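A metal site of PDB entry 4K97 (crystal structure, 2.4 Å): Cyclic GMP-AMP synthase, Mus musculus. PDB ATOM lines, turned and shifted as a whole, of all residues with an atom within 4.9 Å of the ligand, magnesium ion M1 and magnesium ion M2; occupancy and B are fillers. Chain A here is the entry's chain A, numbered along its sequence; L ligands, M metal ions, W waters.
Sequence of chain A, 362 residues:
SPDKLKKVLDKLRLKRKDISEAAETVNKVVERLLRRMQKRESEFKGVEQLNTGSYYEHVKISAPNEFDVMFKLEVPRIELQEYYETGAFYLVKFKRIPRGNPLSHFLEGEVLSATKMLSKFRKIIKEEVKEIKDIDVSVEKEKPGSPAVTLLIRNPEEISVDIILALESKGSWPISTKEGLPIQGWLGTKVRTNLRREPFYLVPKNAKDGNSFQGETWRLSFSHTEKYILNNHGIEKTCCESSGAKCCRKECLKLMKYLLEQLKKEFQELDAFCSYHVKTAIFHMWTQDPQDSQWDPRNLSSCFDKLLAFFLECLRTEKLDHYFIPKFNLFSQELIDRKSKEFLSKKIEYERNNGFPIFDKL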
ATOM      1  N   GLY A  53      26.206  18.886 -18.095  1.00  0.00           N
ATOM      2  CA  GLY A  53      26.582  19.751 -19.216  1.00  0.00           C
ATOM      3  C   GLY A  53      27.498  19.182 -20.285  1.00  0.00           C
ATOM      4  O   GLY A  53      27.854  17.989 -20.268  1.00  0.00           O
ATOM      5  N   SER A  54      27.882  20.057 -21.216  1.00  0.00           N
ATOM      6  CA  SER A  54      28.658  19.720 -22.412  1.00  0.00           C
ATOM      7  C   SER A  54      29.804  18.717 -22.228  1.00  0.00           C
ATOM      8  O   SER A  54      29.829  17.687 -22.899  1.00  0.00           O
ATOM      9  CB  SER A  54      29.195  21.002 -23.049  1.00  0.00           C
ATOM     10  OG  SER A  54      28.620  21.183 -24.325  1.00  0.00           O
ATOM     11  N   GLU A  57      28.700  15.308 -21.168  1.00  0.00           N
ATOM     12  CA  GLU A  57      27.883  14.629 -22.164  1.00  0.00           C
ATOM     13  C   GLU A  57      28.708  14.320 -23.418  1.00  0.00           C
ATOM     14  O   GLU A  57      28.176  13.765 -24.381  1.00  0.00           O
ATOM     15  CB  GLU A  57      26.678  15.485 -22.548  1.00  0.00           C
ATOM     16  CG  GLU A  57      25.756  15.813 -21.389  1.00  0.00           C
ATOM     17  CD  GLU A  57      24.827  16.982 -21.691  1.00  0.00           C
ATOM     18  OE1 GLU A  57      25.250  17.930 -22.391  1.00  0.00           O
ATOM     19  OE2 GLU A  57      23.674  16.960 -21.221  1.00  0.00           O
ATOM     20  N   LYS A  60      31.178  18.843 -25.648  1.00  0.00           N
ATOM     21  CA  LYS A  60      31.988  20.056 -25.541  1.00  0.00           C
ATOM     22  C   LYS A  60      32.860  20.163 -26.786  1.00  0.00           C
ATOM     23  O   LYS A  60      33.440  19.167 -27.234  1.00  0.00           O
ATOM     24  CB  LYS A  60      32.886  19.983 -24.293  1.00  0.00           C
ATOM     25  CG  LYS A  60      33.745  21.234 -24.033  1.00  0.00           C
ATOM     26  CD  LYS A  60      32.869  22.380 -23.519  1.00  0.00           C
ATOM     27  CE  LYS A  60      33.709  23.613 -23.185  1.00  0.00           C
ATOM     28  NZ  LYS A  60      34.135  24.357 -24.396  1.00  0.00           N
ATOM     29  N   GLU A  66      35.204  24.890 -20.172  1.00  0.00           N
ATOM     30  CA  GLU A  66      33.986  25.231 -19.415  1.00  0.00           C
ATOM     31  C   GLU A  66      33.381  23.973 -18.786  1.00  0.00           C
ATOM     32  O   GLU A  66      33.057  23.009 -19.486  1.00  0.00           O
ATOM     33  CB  GLU A  66      32.953  25.956 -20.303  1.00  0.00           C
ATOM     34  CG  GLU A  66      31.977  26.894 -19.554  1.00  0.00           C
ATOM     35  CD  GLU A  66      30.646  26.229 -19.176  1.00  0.00           C
ATOM     36  OE1 GLU A  66      30.416  25.061 -19.548  1.00  0.00           O
ATOM     37  OE2 GLU A  66      29.817  26.895 -18.509  1.00  0.00           O
ATOM     38  N   ASP A  68      30.447  22.379 -15.978  1.00  0.00           N
ATOM     39  CA  ASP A  68      29.267  22.602 -15.140  1.00  0.00           C
ATOM     40  C   ASP A  68      29.152  21.528 -14.067  1.00  0.00           C
ATOM     41  O   ASP A  68      29.298  20.337 -14.355  1.00  0.00           O
ATOM     42  CB  ASP A  68      27.999  22.592 -15.984  1.00  0.00           C
ATOM     43  CG  ASP A  68      28.053  23.595 -17.104  1.00  0.00           C
ATOM     44  OD1 ASP A  68      27.716  24.774 -16.880  1.00  0.00           O
ATOM     45  OD2 ASP A  68      28.463  23.187 -18.212  1.00  0.00           O
ATOM     46  N   ASP A 162      31.134  26.452 -13.556  1.00  0.00           N
ATOM     47  CA  ASP A 162      29.873  26.874 -12.926  1.00  0.00           C
ATOM     48  C   ASP A 162      29.449  25.889 -11.848  1.00  0.00           C
ATOM     49  O   ASP A 162      29.110  24.731 -12.161  1.00  0.00           O
ATOM     50  CB  ASP A 162      28.750  26.993 -13.969  1.00  0.00           C
ATOM     51  CG  ASP A 162      28.983  28.124 -14.967  1.00  0.00           C
ATOM     52  OD1 ASP A 162      29.601  29.140 -14.590  1.00  0.00           O
ATOM     53  OD2 ASP A 162      28.533  28.006 -16.129  1.00  0.00           O
ATOM     54  N   LYS A 205      17.799  30.110 -10.232  1.00  0.00           N
ATOM     55  CA  LYS A 205      17.734  31.055 -11.336  1.00  0.00           C
ATOM     56  C   LYS A 205      16.410  31.815 -11.215  1.00  0.00           C
ATOM     57  O   LYS A 205      15.343  31.196 -11.258  1.00  0.00           O
ATOM     58  CB  LYS A 205      17.832  30.290 -12.660  1.00  0.00           C
ATOM     59  CG  LYS A 205      17.238  30.979 -13.872  1.00  0.00           C
ATOM     60  CD  LYS A 205      18.105  32.108 -14.367  1.00  0.00           C
ATOM     61  CE  LYS A 205      17.838  32.429 -15.836  1.00  0.00           C
ATOM     62  NZ  LYS A 205      18.343  31.361 -16.744  1.00  0.00           N
ATOM     63  N   ARG A 219      13.975  27.703 -10.621  1.00  0.00           N
ATOM     64  CA  ARG A 219      13.719  27.091 -11.923  1.00  0.00           C
ATOM     65  C   ARG A 219      13.906  25.581 -11.965  1.00  0.00           C
ATOM     66  O   ARG A 219      14.781  25.037 -11.368  1.00  0.00           O
ATOM     67  CB  ARG A 219      14.531  27.734 -13.033  1.00  0.00           C
ATOM     68  CG  ARG A 219      13.704  27.949 -14.273  1.00  0.00           C
ATOM     69  CD  ARG A 219      14.442  27.851 -15.585  1.00  0.00           C
ATOM     70  NE  ARG A 219      15.456  26.851 -15.461  1.00  0.00           N
ATOM     71  CZ  ARG A 219      16.686  26.944 -15.926  1.00  0.00           C
ATOM     72  NH1 ARG A 219      17.050  28.026 -16.586  1.00  0.00           N
ATOM     73  NH2 ARG A 219      17.542  25.942 -15.739  1.00  0.00           N
ATOM     74  N   SER A 223      19.073  18.669 -16.133  1.00  0.00           N
ATOM     75  CA  SER A 223      20.441  18.311 -16.487  1.00  0.00           C
ATOM     76  C   SER A 223      20.718  16.810 -16.346  1.00  0.00           C
ATOM     77  O   SER A 223      21.362  16.224 -17.209  1.00  0.00           O
ATOM     78  CB  SER A 223      21.453  19.123 -15.684  1.00  0.00           C
ATOM     79  OG  SER A 223      21.306  20.513 -15.913  1.00  0.00           O
ATOM     80  N   GLU A 226      18.792  14.947 -19.185  1.00  0.00           N
ATOM     81  CA  GLU A 226      19.428  15.249 -20.473  1.00  0.00           C
ATOM     82  C   GLU A 226      20.716  14.458 -20.608  1.00  0.00           C
ATOM     83  O   GLU A 226      21.059  13.995 -21.684  1.00  0.00           O
ATOM     84  CB  GLU A 226      19.702  16.743 -20.598  1.00  0.00           C
ATOM     85  CG  GLU A 226      18.427  17.585 -20.611  1.00  0.00           C
ATOM     86  CD  GLU A 226      18.691  19.070 -20.370  1.00  0.00           C
ATOM     87  OE1 GLU A 226      17.716  19.788 -20.081  1.00  0.00           O
ATOM     88  OE2 GLU A 226      19.855  19.524 -20.467  1.00  0.00           O
ATOM     89  N   LYS A 257      26.200  23.784 -32.539  1.00  0.00           N
ATOM     90  CA  LYS A 257      26.757  24.593 -31.466  1.00  0.00           C
ATOM     91  C   LYS A 257      27.904  25.447 -31.981  1.00  0.00           C
ATOM     92  O   LYS A 257      28.032  26.612 -31.601  1.00  0.00           O
ATOM     93  CB  LYS A 257      27.232  23.736 -30.294  1.00  0.00           C
ATOM     94  CG  LYS A 257      26.136  23.029 -29.557  1.00  0.00           C
ATOM     95  CD  LYS A 257      26.714  22.059 -28.533  1.00  0.00           C
ATOM     96  CE  LYS A 257      27.490  22.807 -27.471  1.00  0.00           C
ATOM     97  NZ  LYS A 257      27.913  21.853 -26.426  1.00  0.00           N
ATOM     98  N   CYS A 274      21.727  30.932 -26.616  1.00  0.00           N
ATOM     99  CA  CYS A 274      22.638  30.077 -25.895  1.00  0.00           C
ATOM    100  C   CYS A 274      22.661  28.703 -26.485  1.00  0.00           C
ATOM    101  O   CYS A 274      21.903  28.401 -27.358  1.00  0.00           O
ATOM    102  CB  CYS A 274      22.286  30.017 -24.425  1.00  0.00           C
ATOM    103  SG  CYS A 274      20.712  29.309 -24.093  1.00  0.00           S
ATOM    104  N   SER A 275      23.582  27.896 -26.043  1.00  0.00           N
ATOM    105  CA  SER A 275      23.684  26.541 -26.521  1.00  0.00           C
ATOM    106  C   SER A 275      22.471  25.705 -26.194  1.00  0.00           C
ATOM    107  O   SER A 275      22.201  24.815 -26.907  1.00  0.00           O
ATOM    108  CB  SER A 275      24.979  25.886 -26.117  1.00  0.00           C
ATOM    109  OG  SER A 275      25.158  25.843 -24.753  1.00  0.00           O
ATOM    110  N   TYR A 276      21.791  25.983 -25.100  1.00  0.00           N
ATOM    111  CA  TYR A 276      20.565  25.246 -24.773  1.00  0.00           C
ATOM    112  C   TYR A 276      19.479  25.321 -25.844  1.00  0.00           C
ATOM    113  O   TYR A 276      18.773  24.347 -26.088  1.00  0.00           O
ATOM    114  CB  TYR A 276      19.976  25.724 -23.447  1.00  0.00           C
ATOM    115  CG  TYR A 276      19.031  24.710 -22.848  1.00  0.00           C
ATOM    116  CD1 TYR A 276      19.502  23.494 -22.393  1.00  0.00           C
ATOM    117  CD2 TYR A 276      17.668  24.974 -22.737  1.00  0.00           C
ATOM    118  CE1 TYR A 276      18.659  22.552 -21.841  1.00  0.00           C
ATOM    119  CE2 TYR A 276      16.813  24.040 -22.185  1.00  0.00           C
ATOM    120  CZ  TYR A 276      17.313  22.831 -21.733  1.00  0.00           C
ATOM    121  OH  TYR A 276      16.481  21.882 -21.181  1.00  0.00           O
ATOM    122  N   LYS A 279      20.477  22.698 -28.157  1.00  0.00           N
ATOM    123  CA  LYS A 279      20.278  21.385 -27.525  1.00  0.00           C
ATOM    124  C   LYS A 279      18.793  21.005 -27.561  1.00  0.00           C
ATOM    125  O   LYS A 279      18.426  19.885 -27.947  1.00  0.00           O
ATOM    126  CB  LYS A 279      20.829  21.420 -26.089  1.00  0.00           C
ATOM    127  CG  LYS A 279      21.068  20.052 -25.435  1.00  0.00           C
ATOM    128  CD  LYS A 279      21.631  20.255 -24.010  1.00  0.00           C
ATOM    129  CE  LYS A 279      21.702  18.962 -23.220  1.00  0.00           C
ATOM    130  NZ  LYS A 279      22.081  19.202 -21.784  1.00  0.00           N
ATOM    131  N   HIS A 322      10.155  24.154 -24.805  1.00  0.00           N
ATOM    132  CA  HIS A 322      11.030  23.468 -23.858  1.00  0.00           C
ATOM    133  C   HIS A 322      10.733  21.967 -23.963  1.00  0.00           C
ATOM    134  O   HIS A 322       9.565  21.575 -23.964  1.00  0.00           O
ATOM    135  CB  HIS A 322      10.764  23.982 -22.441  1.00  0.00           C
ATOM    136  CG  HIS A 322      11.791  23.555 -21.436  1.00  0.00           C
ATOM    137  ND1 HIS A 322      11.966  22.237 -21.075  1.00  0.00           N
ATOM    138  CD2 HIS A 322      12.680  24.278 -20.713  1.00  0.00           C
ATOM    139  CE1 HIS A 322      12.929  22.168 -20.166  1.00  0.00           C
ATOM    140  NE2 HIS A 322      13.379  23.388 -19.930  1.00  0.00           N
HETATM  141  P1  LIG L   1      28.272  24.557 -23.627  1.00  0.00           P
HETATM  142  O1  LIG L   1      29.120  23.821 -24.641  1.00  0.00           O
HETATM  143  O2  LIG L   1      28.892  24.624 -22.251  1.00  0.00           O
HETATM  144  O3  LIG L   1      27.778  25.899 -24.105  1.00  0.00           O
HETATM  145  P2  LIG L   1      26.252  23.341 -22.038  1.00  0.00           P
HETATM  146  O4  LIG L   1      27.285  22.939 -21.016  1.00  0.00           O
HETATM  147  O5  LIG L   1      25.073  22.435 -22.312  1.00  0.00           O
HETATM  148  O6  LIG L   1      26.939  23.663 -23.475  1.00  0.00           O
HETATM  149  P3  LIG L   1      25.698  25.670 -20.374  1.00  0.00           P
HETATM  150  O7  LIG L   1      27.078  25.531 -19.763  1.00  0.00           O
HETATM  151  O8  LIG L   1      25.141  27.017 -20.757  1.00  0.00           O
HETATM  152  O9  LIG L   1      25.619  24.807 -21.732  1.00  0.00           O
HETATM  153  O10 LIG L   1      24.604  25.031 -19.372  1.00  0.00           O
HETATM  154  C1  LIG L   1      24.884  23.835 -18.640  1.00  0.00           C
HETATM  155  C2  LIG L   1      23.570  23.066 -18.424  1.00  0.00           C
HETATM  156  O11 LIG L   1      22.606  23.821 -17.675  1.00  0.00           O
HETATM  157  C3  LIG L   1      22.910  22.715 -19.743  1.00  0.00           C
HETATM  158  O12 LIG L   1      23.370  21.457 -20.241  1.00  0.00           O
HETATM  159  C4  LIG L   1      21.425  22.681 -19.406  1.00  0.00           C
HETATM  160  O13 LIG L   1      21.004  21.375 -18.998  1.00  0.00           O
HETATM  161  C5  LIG L   1      21.291  23.660 -18.235  1.00  0.00           C
HETATM  162  N1  LIG L   1      20.811  24.945 -18.809  1.00  0.00           N
HETATM  163  C6  LIG L   1      21.603  25.949 -19.223  1.00  0.00           C
HETATM  164  N2  LIG L   1      20.872  26.985 -19.707  1.00  0.00           N
HETATM  165  C7  LIG L   1      19.576  26.653 -19.613  1.00  0.00           C
HETATM  166  C8  LIG L   1      18.290  27.307 -19.947  1.00  0.00           C
HETATM  167  N3  LIG L   1      18.266  28.552 -20.503  1.00  0.00           N
HETATM  168  N4  LIG L   1      17.148  26.616 -19.693  1.00  0.00           N
HETATM  169  C9  LIG L   1      17.181  25.372 -19.148  1.00  0.00           C
HETATM  170  N5  LIG L   1      18.320  24.723 -18.822  1.00  0.00           N
HETATM  171  C10 LIG L   1      19.526  25.301 -19.018  1.00  0.00           C
HETATM  172 MG    MG M   1      27.773  26.711 -17.755  1.00  0.00          MG
HETATM  173 MG    MG M   2      28.886  24.062 -20.206  1.00  0.00          MG
HETATM  174  O   HOH W   1      23.509  23.214 -23.971  1.00  0.00           O
HETATM  175  O   HOH W   2      25.298  27.420 -16.837  1.00  0.00           O
HETATM  176  O   HOH W   3      21.834  29.297 -20.184  1.00  0.00           O
HETATM  177  O   HOH W   4      30.520  22.295 -20.509  1.00  0.00           O
HETATM  178  O   HOH W   5      23.546  27.517 -22.552  1.00  0.00           O
HETATM  179  O   HOH W   6      20.122  25.043 -15.250  1.00  0.00           O
HETATM  180  O   HOH W   7      28.078  28.472 -19.387  1.00  0.00           O
HETATM  181  O   HOH W   8      31.279  24.209 -26.367  1.00  0.00           O
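Magnesium ion M1 is bound by OD1 of Asp 68 (2.1 Å), OE2 of Glu 66 (2.2 Å), OD2 of Asp 162 (2.2 Å), water W7 (2.4 Å) and O7 of the ligand (2.4 Å).
Magnesium ion M1 has five donor atoms within binding distance.
Slightly farther from magnesium ion M1 lies water W2 (2.7 Å).
Water W1 lies within hydrogen-bond range of O5 of the ligand, OG of Ser 275 and N of Tyr 276.
Water W5 lies within hydrogen-bond range of O8 of the ligand (2.5 Å), OG of Ser 275 (3.2 Å), N of Tyr 276 (3.5 Å) and SG of Cys 274 (3.7 Å).
Water W8 bridges an oxygen (O1) of the ligand (2.8 Å) and the side-chain amino group of Lys 60 (3.5 Å).
The side-chain amino group of Lys 279 lies within salt-bridge range of the side-chain carboxylate of Glu 226 (2.6 Å).
The side-chain carboxylate of Glu 226 is in hydrogen-bond range of the side-chain hydroxyl of Tyr 276, at 2.7 Å.
N of Lys 60 lies within hydrogen-bond range of O of Ser 54 (3.3 Å).
NZ of Lys 279 is in salt-bridge range of OE2 of Glu 57 (2.8 Å).
SG of Cys 274 sits close to N of Tyr 276.
The side-chain carboxylate (OE2) of Glu 226 lies within hydrogen-bond range of an oxygen (O13) of the ligand (2.6 Å).
The side-chain hydroxyl (OG) of Ser 275 sits at hydrogen-bond distance from an oxygen (O3) of the ligand (2.7 Å).
The backbone NH (N) of Ser 54 sits close to an oxygen (O4) of the ligand, at 2.9 Å.
O1 of the ligand is in hydrogen-bond range of OG of Ser 54 (2.7 Å).
NZ of Lys 257 lies within salt-bridge range of O1 of the ligand, at 2.9 Å.
The side-chain amino group of Lys 279 lies within hydrogen-bond range of an oxygen (O12) of the ligand.
OG of Ser 223 is in hydrogen-bond range of O13 of the ligand.
The guanidinium group (NH2) of Arg 219 lies within hydrogen-bond range of a nitrogen (N5) of the ligand (3.4 Å).
Magnesium ion M2 is bound by the side-chain carboxylate of Glu 66 (1.9 Å), an oxygen (O4) of the ligand (2.1 Å), an oxygen (O2) of the ligand (2.1 Å), the side-chain carboxylate of Asp 68 (2.2 Å), an oxygen (O7) of the ligand (2.4 Å) and water W4 (2.4 Å).
Magnesium ion M2 has six donor atoms within binding distance.
The nearest printed residue that does not touch magnesium ion M1 is Gly 53 (7.2 Å).
Residues that only touch the ligand: Tyr 276 and Gly 53.
Hydrophobic or aromatic side chains within 4 Å of the ligand: Tyr 276.
Of the 17 residues printed, 11 come within 4 Å of the ligand.
Along chain A the residues within 4 Å of the ligand span positions 53 to 279.
Within 4 Å of magnesium ion M2: Glu 66 and Asp 68.
The nearest printed residue that does not touch magnesium ion M2 is Ser 54 (4.2 Å).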
